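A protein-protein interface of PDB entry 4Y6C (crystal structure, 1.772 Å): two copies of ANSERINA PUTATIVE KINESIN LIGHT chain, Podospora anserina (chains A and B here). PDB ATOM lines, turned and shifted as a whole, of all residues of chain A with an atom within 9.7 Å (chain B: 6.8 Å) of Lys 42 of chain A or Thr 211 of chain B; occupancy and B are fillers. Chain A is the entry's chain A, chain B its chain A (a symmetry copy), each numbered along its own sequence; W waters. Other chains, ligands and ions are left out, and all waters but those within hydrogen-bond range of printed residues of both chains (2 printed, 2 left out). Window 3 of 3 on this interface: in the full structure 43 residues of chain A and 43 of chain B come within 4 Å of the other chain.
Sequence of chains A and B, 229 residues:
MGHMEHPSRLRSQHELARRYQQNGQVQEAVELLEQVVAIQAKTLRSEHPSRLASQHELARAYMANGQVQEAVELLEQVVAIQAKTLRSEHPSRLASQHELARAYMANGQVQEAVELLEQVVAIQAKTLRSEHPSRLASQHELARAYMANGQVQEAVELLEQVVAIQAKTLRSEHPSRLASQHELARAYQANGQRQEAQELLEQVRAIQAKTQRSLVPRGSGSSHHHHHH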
ATOM      1  N   HIS A   3      24.289   3.315   0.271  1.00  0.00           N
ATOM      2  CA  HIS A   3      24.799   2.249  -0.579  1.00  0.00           C
ATOM      3  C   HIS A   3      25.690   1.298   0.227  1.00  0.00           C
ATOM      4  O   HIS A   3      25.886   0.147  -0.159  1.00  0.00           O
ATOM      5  CB  HIS A   3      25.558   2.839  -1.776  1.00  0.00           C
ATOM      6  CG  HIS A   3      26.231   1.814  -2.636  1.00  0.00           C
ATOM      7  ND1 HIS A   3      27.525   1.956  -3.092  1.00  0.00           N
ATOM      8  CD2 HIS A   3      25.789   0.633  -3.128  1.00  0.00           C
ATOM      9  CE1 HIS A   3      27.850   0.906  -3.823  1.00  0.00           C
ATOM     10  NE2 HIS A   3      26.814   0.086  -3.859  1.00  0.00           N
ATOM     11  N   MET A   4      26.236   1.786   1.339  1.00  0.00           N
ATOM     12  CA  MET A   4      26.984   0.957   2.285  1.00  0.00           C
ATOM     13  C   MET A   4      26.102  -0.217   2.711  1.00  0.00           C
ATOM     14  O   MET A   4      24.907  -0.028   2.935  1.00  0.00           O
ATOM     15  CB  MET A   4      27.420   1.816   3.482  1.00  0.00           C
ATOM     16  CG  MET A   4      27.793   1.091   4.752  1.00  0.00           C
ATOM     17  SD  MET A   4      28.006   2.421   6.203  1.00  0.00           S
ATOM     18  CE  MET A   4      29.229   3.655   5.276  1.00  0.00           C
ATOM     19  N   PRO A   7      24.243  -0.105   7.056  1.00  0.00           N
ATOM     20  CA  PRO A   7      24.269   1.211   7.719  1.00  0.00           C
ATOM     21  C   PRO A   7      23.874   1.175   9.198  1.00  0.00           C
ATOM     22  O   PRO A   7      24.294   2.050   9.953  1.00  0.00           O
ATOM     23  CB  PRO A   7      23.262   2.038   6.902  1.00  0.00           C
ATOM     24  CG  PRO A   7      22.443   1.033   6.135  1.00  0.00           C
ATOM     25  CD  PRO A   7      23.359  -0.121   5.879  1.00  0.00           C
ATOM     26  N   LEU A  10      26.587   1.335  11.985  1.00  0.00           N
ATOM     27  CA  LEU A  10      27.307   2.565  12.294  1.00  0.00           C
ATOM     28  C   LEU A  10      27.147   2.982  13.753  1.00  0.00           C
ATOM     29  O   LEU A  10      27.728   3.980  14.182  1.00  0.00           O
ATOM     30  CB  LEU A  10      26.848   3.698  11.378  1.00  0.00           C
ATOM     31  CG  LEU A  10      27.426   3.679   9.962  1.00  0.00           C
ATOM     32  CD1 LEU A  10      26.800   4.785   9.129  1.00  0.00           C
ATOM     33  CD2 LEU A  10      28.956   3.805   9.972  1.00  0.00           C
ATOM     34  N   GLU A  31      30.760  16.221  14.251  1.00  0.00           N
ATOM     35  CA  GLU A  31      31.049  15.971  12.840  1.00  0.00           C
ATOM     36  C   GLU A  31      30.917  14.490  12.497  1.00  0.00           C
ATOM     37  O   GLU A  31      30.359  14.134  11.458  1.00  0.00           O
ATOM     38  CB  GLU A  31      32.453  16.455  12.483  1.00  0.00           C
ATOM     39  CG  GLU A  31      32.673  17.938  12.725  1.00  0.00           C
ATOM     40  CD  GLU A  31      32.105  18.800  11.618  1.00  0.00           C
ATOM     41  OE1 GLU A  31      31.900  18.278  10.501  1.00  0.00           O
ATOM     42  OE2 GLU A  31      31.866  20.003  11.865  1.00  0.00           O
ATOM     43  N   LEU A  32      31.447  13.639  13.370  1.00  0.00           N
ATOM     44  CA  LEU A  32      31.379  12.191  13.184  1.00  0.00           C
ATOM     45  C   LEU A  32      29.934  11.719  13.096  1.00  0.00           C
ATOM     46  O   LEU A  32      29.565  10.976  12.185  1.00  0.00           O
ATOM     47  CB  LEU A  32      32.090  11.468  14.336  1.00  0.00           C
ATOM     48  CG  LEU A  32      32.270   9.947  14.225  1.00  0.00           C
ATOM     49  CD1 LEU A  32      33.386   9.574  13.262  1.00  0.00           C
ATOM     50  CD2 LEU A  32      32.525   9.314  15.602  1.00  0.00           C
ATOM     51  N   LEU A  33      29.111  12.154  14.046  1.00  0.00           N
ATOM     52  CA  LEU A  33      27.752  11.627  14.126  1.00  0.00           C
ATOM     53  C   LEU A  33      26.808  12.291  13.135  1.00  0.00           C
ATOM     54  O   LEU A  33      25.798  11.698  12.755  1.00  0.00           O
ATOM     55  CB  LEU A  33      27.215  11.765  15.547  1.00  0.00           C
ATOM     56  CG  LEU A  33      27.980  10.912  16.558  1.00  0.00           C
ATOM     57  CD1 LEU A  33      27.381  11.086  17.952  1.00  0.00           C
ATOM     58  CD2 LEU A  33      27.947   9.446  16.135  1.00  0.00           C
ATOM     59  N   GLU A  34      27.122  13.510  12.708  1.00  0.00           N
ATOM     60  CA  GLU A  34      26.347  14.118  11.621  1.00  0.00           C
ATOM     61  C   GLU A  34      26.485  13.287  10.359  1.00  0.00           C
ATOM     62  O   GLU A  34      25.537  13.163   9.582  1.00  0.00           O
ATOM     63  CB  GLU A  34      26.795  15.562  11.353  1.00  0.00           C
ATOM     64  CG  GLU A  34      26.171  16.557  12.322  1.00  0.00           C
ATOM     65  CD  GLU A  34      26.638  17.986  12.113  1.00  0.00           C
ATOM     66  OE1 GLU A  34      27.750  18.185  11.582  1.00  0.00           O
ATOM     67  OE2 GLU A  34      25.889  18.917  12.496  1.00  0.00           O
ATOM     68  N   GLN A  35      27.669  12.717  10.147  1.00  0.00           N
ATOM     69  CA  GLN A  35      27.884  11.892   8.965  1.00  0.00           C
ATOM     70  C   GLN A  35      27.155  10.549   9.105  1.00  0.00           C
ATOM     71  O   GLN A  35      26.574  10.048   8.134  1.00  0.00           O
ATOM     72  CB  GLN A  35      29.382  11.683   8.713  1.00  0.00           C
ATOM     73  CG  GLN A  35      29.714  10.868   7.451  1.00  0.00           C
ATOM     74  CD  GLN A  35      29.560  11.643   6.150  1.00  0.00           C
ATOM     75  OE1 GLN A  35      29.138  12.795   6.135  1.00  0.00           O
ATOM     76  NE2 GLN A  35      29.917  11.001   5.045  1.00  0.00           N
ATOM     77  N   VAL A  36      27.178   9.963  10.304  1.00  0.00           N
ATOM     78  CA  VAL A  36      26.401   8.743  10.564  1.00  0.00           C
ATOM     79  C   VAL A  36      24.923   8.975  10.250  1.00  0.00           C
ATOM     80  O   VAL A  36      24.289   8.197   9.541  1.00  0.00           O
ATOM     81  CB  VAL A  36      26.530   8.276  12.036  1.00  0.00           C
ATOM     82  CG1 VAL A  36      25.479   7.206  12.376  1.00  0.00           C
ATOM     83  CG2 VAL A  36      27.938   7.770  12.319  1.00  0.00           C
ATOM     84  N   VAL A  37      24.386  10.064  10.783  1.00  0.00           N
ATOM     85  CA  VAL A  37      22.963  10.342  10.661  1.00  0.00           C
ATOM     86  C   VAL A  37      22.604  10.584   9.194  1.00  0.00           C
ATOM     87  O   VAL A  37      21.553  10.123   8.721  1.00  0.00           O
ATOM     88  CB  VAL A  37      22.555  11.535  11.564  1.00  0.00           C
ATOM     89  CG1 VAL A  37      21.199  12.116  11.155  1.00  0.00           C
ATOM     90  CG2 VAL A  37      22.529  11.083  13.020  1.00  0.00           C
ATOM     91  N   ALA A  38      23.486  11.258   8.459  1.00  0.00           N
ATOM     92  CA  ALA A  38      23.218  11.508   7.041  1.00  0.00           C
ATOM     93  C   ALA A  38      23.226  10.216   6.228  1.00  0.00           C
ATOM     94  O   ALA A  38      22.414  10.048   5.322  1.00  0.00           O
ATOM     95  CB  ALA A  38      24.232  12.510   6.461  1.00  0.00           C
ATOM     96  N   ILE A  39      24.140   9.301   6.546  1.00  0.00           N
ATOM     97  CA  ILE A  39      24.207   8.027   5.827  1.00  0.00           C
ATOM     98  C   ILE A  39      22.959   7.189   6.106  1.00  0.00           C
ATOM     99  O   ILE A  39      22.344   6.625   5.193  1.00  0.00           O
ATOM    100  CB  ILE A  39      25.459   7.231   6.225  1.00  0.00           C
ATOM    101  CG1 ILE A  39      26.712   7.949   5.726  1.00  0.00           C
ATOM    102  CG2 ILE A  39      25.387   5.817   5.671  1.00  0.00           C
ATOM    103  CD1 ILE A  39      28.033   7.359   6.264  1.00  0.00           C
ATOM    104  N   GLN A  40      22.577   7.112   7.375  1.00  0.00           N
ATOM    105  CA  GLN A  40      21.406   6.317   7.737  1.00  0.00           C
ATOM    106  C   GLN A  40      20.099   6.930   7.208  1.00  0.00           C
ATOM    107  O   GLN A  40      19.128   6.215   6.969  1.00  0.00           O
ATOM    108  CB  GLN A  40      21.342   6.150   9.250  1.00  0.00           C
ATOM    109  CG  GLN A  40      22.487   5.313   9.776  1.00  0.00           C
ATOM    110  CD  GLN A  40      22.383   5.059  11.263  1.00  0.00           C
ATOM    111  OE1 GLN A  40      21.795   5.853  11.998  1.00  0.00           O
ATOM    112  NE2 GLN A  40      22.946   3.943  11.712  1.00  0.00           N
ATOM    113  N   ALA A  41      20.073   8.243   7.008  1.00  0.00           N
ATOM    114  CA  ALA A  41      18.853   8.888   6.504  1.00  0.00           C
ATOM    115  C   ALA A  41      18.542   8.430   5.085  1.00  0.00           C
ATOM    116  O   ALA A  41      17.394   8.503   4.641  1.00  0.00           O
ATOM    117  CB  ALA A  41      18.980  10.406   6.549  1.00  0.00           C
ATOM    118  N   LYS A  42      19.568   7.971   4.369  1.00  0.00           N
ATOM    119  CA  LYS A  42      19.405   7.598   2.966  1.00  0.00           C
ATOM    120  C   LYS A  42      18.989   6.151   2.806  1.00  0.00           C
ATOM    121  O   LYS A  42      18.610   5.735   1.713  1.00  0.00           O
ATOM    122  CB  LYS A  42      20.705   7.827   2.190  1.00  0.00           C
ATOM    123  CG  LYS A  42      21.141   9.287   2.120  1.00  0.00           C
ATOM    124  CD  LYS A  42      22.359   9.423   1.205  1.00  0.00           C
ATOM    125  CE  LYS A  42      23.082  10.736   1.442  1.00  0.00           C
ATOM    126  NZ  LYS A  42      22.174  11.891   1.222  1.00  0.00           N
ATOM    127  N   THR A  43      19.068   5.385   3.893  1.00  0.00           N
ATOM    128  CA  THR A  43      18.996   3.937   3.789  1.00  0.00           C
ATOM    129  C   THR A  43      17.987   3.292   4.750  1.00  0.00           C
ATOM    130  O   THR A  43      17.434   2.236   4.442  1.00  0.00           O
ATOM    131  CB  THR A  43      20.396   3.318   4.023  1.00  0.00           C
ATOM    132  OG1 THR A  43      20.940   3.818   5.253  1.00  0.00           O
ATOM    133  CG2 THR A  43      21.338   3.717   2.901  1.00  0.00           C
ATOM    134  N   LEU A  44      17.740   3.933   5.893  1.00  0.00           N
ATOM    135  CA  LEU A  44      16.893   3.357   6.946  1.00  0.00           C
ATOM    136  C   LEU A  44      15.602   4.149   7.123  1.00  0.00           C
ATOM    137  O   LEU A  44      15.617   5.369   7.043  1.00  0.00           O
ATOM    138  CB  LEU A  44      17.649   3.326   8.282  1.00  0.00           C
ATOM    139  CG  LEU A  44      18.945   2.514   8.325  1.00  0.00           C
ATOM    140  CD1 LEU A  44      19.594   2.617   9.715  1.00  0.00           C
ATOM    141  CD2 LEU A  44      18.647   1.067   7.969  1.00  0.00           C
ATOM    142  N   ARG A  45      14.489   3.465   7.376  1.00  0.00           N
ATOM    143  CA  ARG A  45      13.217   4.163   7.589  1.00  0.00           C
ATOM    144  C   ARG A  45      13.253   4.975   8.878  1.00  0.00           C
ATOM    145  O   ARG A  45      14.029   4.673   9.784  1.00  0.00           O
ATOM    146  CB  ARG A  45      12.056   3.162   7.609  1.00  0.00           C
ATOM    147  CG  ARG A  45      11.847   2.509   6.249  1.00  0.00           C
ATOM    148  CD  ARG A  45      10.689   1.506   6.204  1.00  0.00           C
ATOM    149  NE  ARG A  45      10.936   0.370   7.081  1.00  0.00           N
ATOM    150  CZ  ARG A  45      10.325   0.179   8.242  1.00  0.00           C
ATOM    151  NH1 ARG A  45       9.394   1.028   8.641  1.00  0.00           N
ATOM    152  NH2 ARG A  45      10.621  -0.880   8.983  1.00  0.00           N
ATOM    153  N   SER A  46      12.407   6.002   8.960  1.00  0.00           N
ATOM    154  CA  SER A  46      12.417   6.902  10.113  1.00  0.00           C
ATOM    155  C   SER A  46      12.125   6.184  11.427  1.00  0.00           C
ATOM    156  O   SER A  46      12.553   6.650  12.471  1.00  0.00           O
ATOM    157  CB  SER A  46      11.408   8.034   9.918  1.00  0.00           C
ATOM    158  OG  SER A  46      10.107   7.521   9.684  1.00  0.00           O
ATOM    159  N   ARG A  51      18.341   3.941  13.407  1.00  0.00           N
ATOM    160  CA  ARG A  51      18.360   5.311  12.917  1.00  0.00           C
ATOM    161  C   ARG A  51      18.031   6.282  14.054  1.00  0.00           C
ATOM    162  O   ARG A  51      18.715   7.288  14.247  1.00  0.00           O
ATOM    163  CB  ARG A  51      17.385   5.492  11.748  1.00  0.00           C
ATOM    164  CG  ARG A  51      17.391   6.925  11.206  1.00  0.00           C
ATOM    165  CD  ARG A  51      16.637   7.055   9.872  1.00  0.00           C
ATOM    166  NE  ARG A  51      16.568   8.465   9.496  1.00  0.00           N
ATOM    167  CZ  ARG A  51      15.824   8.965   8.516  1.00  0.00           C
ATOM    168  NH1 ARG A  51      15.088   8.164   7.761  1.00  0.00           N
ATOM    169  NH2 ARG A  51      15.839  10.277   8.281  1.00  0.00           N
ATOM    170  N   SER B 172      34.606   5.777   1.068  1.00  0.00           N
ATOM    171  CA  SER B 172      35.111   7.133   1.259  1.00  0.00           C
ATOM    172  C   SER B 172      34.217   7.949   2.204  1.00  0.00           C
ATOM    173  O   SER B 172      34.690   8.871   2.867  1.00  0.00           O
ATOM    174  CB  SER B 172      35.262   7.847  -0.081  1.00  0.00           C
ATOM    175  OG  SER B 172      34.005   8.124  -0.653  1.00  0.00           O
ATOM    176  N   GLU B 173      32.938   7.588   2.282  1.00  0.00           N
ATOM    177  CA  GLU B 173      31.978   8.358   3.075  1.00  0.00           C
ATOM    178  C   GLU B 173      31.932   7.911   4.536  1.00  0.00           C
ATOM    179  O   GLU B 173      31.299   8.562   5.361  1.00  0.00           O
ATOM    180  CB  GLU B 173      30.575   8.256   2.455  1.00  0.00           C
ATOM    181  CG  GLU B 173      29.928   6.890   2.670  1.00  0.00           C
ATOM    182  CD  GLU B 173      28.631   6.706   1.905  1.00  0.00           C
ATOM    183  OE1 GLU B 173      28.131   7.696   1.329  1.00  0.00           O
ATOM    184  OE2 GLU B 173      28.110   5.570   1.884  1.00  0.00           O
ATOM    185  N   LEU B 178      36.747   9.520   7.338  1.00  0.00           N
ATOM    186  CA  LEU B 178      36.817  10.983   7.351  1.00  0.00           C
ATOM    187  C   LEU B 178      37.492  11.507   8.619  1.00  0.00           C
ATOM    188  O   LEU B 178      38.276  12.454   8.568  1.00  0.00           O
ATOM    189  CB  LEU B 178      35.414  11.573   7.220  1.00  0.00           C
ATOM    190  CG  LEU B 178      34.761  11.218   5.886  1.00  0.00           C
ATOM    191  CD1 LEU B 178      33.287  11.579   5.937  1.00  0.00           C
ATOM    192  CD2 LEU B 178      35.453  11.958   4.757  1.00  0.00           C
ATOM    193  N   ALA B 206      34.449  18.173   1.184  1.00  0.00           N
ATOM    194  CA  ALA B 206      33.691  17.866  -0.021  1.00  0.00           C
ATOM    195  C   ALA B 206      32.846  16.607   0.152  1.00  0.00           C
ATOM    196  O   ALA B 206      31.704  16.558  -0.301  1.00  0.00           O
ATOM    197  CB  ALA B 206      34.620  17.715  -1.219  1.00  0.00           C
ATOM    198  N   ILE B 207      33.402  15.585   0.795  1.00  0.00           N
ATOM    199  CA  ILE B 207      32.666  14.337   0.968  1.00  0.00           C
ATOM    200  C   ILE B 207      31.545  14.533   1.980  1.00  0.00           C
ATOM    201  O   ILE B 207      30.427  14.046   1.784  1.00  0.00           O
ATOM    202  CB  ILE B 207      33.599  13.185   1.399  1.00  0.00           C
ATOM    203  CG1 ILE B 207      34.527  12.821   0.236  1.00  0.00           C
ATOM    204  CG2 ILE B 207      32.793  11.957   1.814  1.00  0.00           C
ATOM    205  CD1 ILE B 207      35.614  11.836   0.621  1.00  0.00           C
ATOM    206  N   GLN B 208      31.825  15.277   3.049  1.00  0.00           N
ATOM    207  CA  GLN B 208      30.793  15.594   4.033  1.00  0.00           C
ATOM    208  C   GLN B 208      29.630  16.349   3.398  1.00  0.00           C
ATOM    209  O   GLN B 208      28.462  16.065   3.670  1.00  0.00           O
ATOM    210  CB  GLN B 208      31.383  16.407   5.186  1.00  0.00           C
ATOM    211  CG  GLN B 208      32.306  15.599   6.085  1.00  0.00           C
ATOM    212  CD  GLN B 208      33.078  16.476   7.048  1.00  0.00           C
ATOM    213  OE1 GLN B 208      33.341  17.646   6.763  1.00  0.00           O
ATOM    214  NE2 GLN B 208      33.429  15.921   8.202  1.00  0.00           N
ATOM    215  N   ALA B 209      29.950  17.303   2.532  1.00  0.00           N
ATOM    216  CA  ALA B 209      28.922  18.111   1.893  1.00  0.00           C
ATOM    217  C   ALA B 209      28.056  17.262   0.968  1.00  0.00           C
ATOM    218  O   ALA B 209      26.841  17.446   0.888  1.00  0.00           O
ATOM    219  CB  ALA B 209      29.559  19.253   1.126  1.00  0.00           C
ATOM    220  N   LYS B 210      28.688  16.330   0.268  1.00  0.00           N
ATOM    221  CA  LYS B 210      27.978  15.516  -0.706  1.00  0.00           C
ATOM    222  C   LYS B 210      27.048  14.542   0.011  1.00  0.00           C
ATOM    223  O   LYS B 210      25.957  14.246  -0.465  1.00  0.00           O
ATOM    224  CB  LYS B 210      28.972  14.787  -1.607  1.00  0.00           C
ATOM    225  CG  LYS B 210      28.366  13.708  -2.485  1.00  0.00           C
ATOM    226  CD  LYS B 210      29.418  13.067  -3.392  1.00  0.00           C
ATOM    227  CE  LYS B 210      30.816  13.121  -2.781  1.00  0.00           C
ATOM    228  NZ  LYS B 210      31.145  11.891  -2.010  1.00  0.00           N
ATOM    229  N   THR B 211      27.471  14.078   1.180  1.00  0.00           N
ATOM    230  CA  THR B 211      26.659  13.144   1.953  1.00  0.00           C
ATOM    231  C   THR B 211      25.521  13.848   2.687  1.00  0.00           C
ATOM    232  O   THR B 211      24.387  13.364   2.723  1.00  0.00           O
ATOM    233  CB  THR B 211      27.529  12.397   2.979  1.00  0.00           C
ATOM    234  OG1 THR B 211      28.670  11.830   2.321  1.00  0.00           O
ATOM    235  CG2 THR B 211      26.731  11.284   3.666  1.00  0.00           C
ATOM    236  N   GLN B 212      25.838  14.997   3.278  1.00  0.00           N
ATOM    237  CA  GLN B 212      24.935  15.658   4.213  1.00  0.00           C
ATOM    238  C   GLN B 212      24.050  16.712   3.569  1.00  0.00           C
ATOM    239  O   GLN B 212      23.005  17.069   4.105  1.00  0.00           O
ATOM    240  CB  GLN B 212      25.745  16.293   5.343  1.00  0.00           C
ATOM    241  CG  GLN B 212      26.542  15.279   6.145  1.00  0.00           C
ATOM    242  CD  GLN B 212      27.389  15.924   7.220  1.00  0.00           C
ATOM    243  OE1 GLN B 212      27.046  16.980   7.742  1.00  0.00           O
ATOM    244  NE2 GLN B 212      28.506  15.298   7.544  1.00  0.00           N
ATOM    245  N   ARG B 213      24.480  17.221   2.424  1.00  0.00           N
ATOM    246  CA  ARG B 213      23.719  18.233   1.705  1.00  0.00           C
ATOM    247  C   ARG B 213      23.760  17.891   0.226  1.00  0.00           C
ATOM    248  O   ARG B 213      24.238  18.681  -0.588  1.00  0.00           O
ATOM    249  CB  ARG B 213      24.288  19.629   1.962  1.00  0.00           C
ATOM    250  CG  ARG B 213      24.605  19.911   3.427  1.00  0.00           C
ATOM    251  CD  ARG B 213      25.350  21.221   3.614  1.00  0.00           C
ATOM    252  NE  ARG B 213      26.730  20.979   4.029  1.00  0.00           N
ATOM    253  CZ  ARG B 213      27.098  20.632   5.259  1.00  0.00           C
ATOM    254  NH1 ARG B 213      26.188  20.489   6.216  1.00  0.00           N
ATOM    255  NH2 ARG B 213      28.380  20.430   5.533  1.00  0.00           N
ATOM    256  N   SER B 214      23.272  16.696  -0.099  1.00  0.00           N
ATOM    257  CA  SER B 214      23.308  16.185  -1.466  1.00  0.00           C
ATOM    258  C   SER B 214      22.562  17.095  -2.433  1.00  0.00           C
ATOM    259  O   SER B 214      23.051  17.382  -3.523  1.00  0.00           O
ATOM    260  CB  SER B 214      22.721  14.772  -1.526  1.00  0.00           C
ATOM    261  OG  SER B 214      22.655  14.305  -2.863  1.00  0.00           O
HETATM  262  O   HOH W   1      32.185  13.453   9.157  1.00  0.00           O
HETATM  263  O   HOH W   2      21.960  14.755   1.872  1.00  0.00           O
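O of Glu 173 of chain B is in hydrogen-bond range of NE2 of Gln 35 of chain A (2.8 Å).
O of Thr 211 of chain B lies within hydrogen-bond range of NZ of Lys 42 of chain A (3.1 Å).
OE1 of Gln 35 of chain A lies within hydrogen-bond range of NE2 of Gln 212 of chain B (2.9 Å).
The side-chain amide nitrogen of Gln 35 of chain A is in hydrogen-bond range of the side-chain hydroxyl of Thr 211 of chain B, at 3.1 Å.
The backbone carbonyl oxygen of Ile 39 of chain A sits at hydrogen-bond distance from the side-chain hydroxyl of Thr 43 of chain A.
The side-chain hydroxyl of Thr 211 of chain B lies within hydrogen-bond range of the backbone carbonyl oxygen of Ile 207 of chain B, 2.9 Å away.
Among the printed residues, pairs that only touch across the chains: Glu 31 of chain A with Gln 208 of chain B (3.6 Å), Glu 34 of chain A with Gln 212 of chain B (3.9 Å), Gln 35 of chain A with Leu 178 of chain B (3.5 Å), Gln 35 of chain A with Gln 208 of chain B (3.9 Å), Ala 38 of chain A with Thr 211 of chain B (3.8 Å), Ala 38 of chain A with Gln 212 of chain B (3.6 Å), Ile 39 of chain A with Glu 173 of chain B (3.6 Å) and Ile 39 of chain A with Thr 211 of chain B (3.9 Å).
Of the printed residues of chain B, Glu 31 of chain A touches Gln 208 (3.6 Å).
Of the printed residues of chain B, Glu 34 of chain A touches Gln 212.
Printed residues of chain B within 4 Å of Gln 35 of chain A: Glu 173, Leu 178, Gln 208, Thr 211 and Gln 212.
Printed residues of chain B within 4 Å of Ala 38 of chain A: Thr 211 (3.8 Å) and Gln 212 (3.6 Å).
Printed residues of chain B within 4 Å of Lys 42 of chain A: Thr 211.
No residue of chain A comes within 4 Å of Ala 209 of chain B.
No residue of chain A comes within 4 Å of Lys 210 of chain B.
Of the printed residues of chain A, Gln 212 of chain B touches Glu 34 (3.9 Å), Gln 35 (2.9 Å) and Ala 38 (3.6 Å).
The nearest printed residue of chain B that does not touch Lys 42 of chain A is Ser 214 of chain B (4.02 Å).
The nearest residue of chain A that does not touch Thr 211 of chain B is Glu 34 of chain A (6.3 Å).
Of the 21 printed residues of chain A, 6 touch a printed residue of chain B.
Hydrophobic or aromatic side chains of chain A that line the printed part of chain B: Ala 38 and Ile 39.
Of the 12 printed residues of chain B, 5 touch a printed residue of chain A.
Printed residues of chain B that touch a printed residue of chain A: Glu 173, Leu 178, Gln 208, Thr 211 and Gln 212.
Hydrophobic or aromatic side chains of chain B within 4 Å of the printed part of chain A: Leu 178.
Among the printed residues, no Asp or Glu carboxylate lies within 4 Å of a Lys or Arg side-chain nitrogen of the other chain.
No position is printed for both chains.
Of the 12 pairs that touch across the chains among the printed residues, none has its exchanged pair printed and touching as well.
Water W2 lies within hydrogen-bond range of the backbone carbonyl oxygen of Thr 211 of chain B, the side-chain amino group of Lys 42 of chain A, the backbone NH of Ser 214 of chain B and the backbone carbonyl oxygen of Gln 212 of chain B.
Water W1 bridges NE2 of Gln 208 of chain B (2.9 Å) and O of Glu 31 of chain A (3.0 Å).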
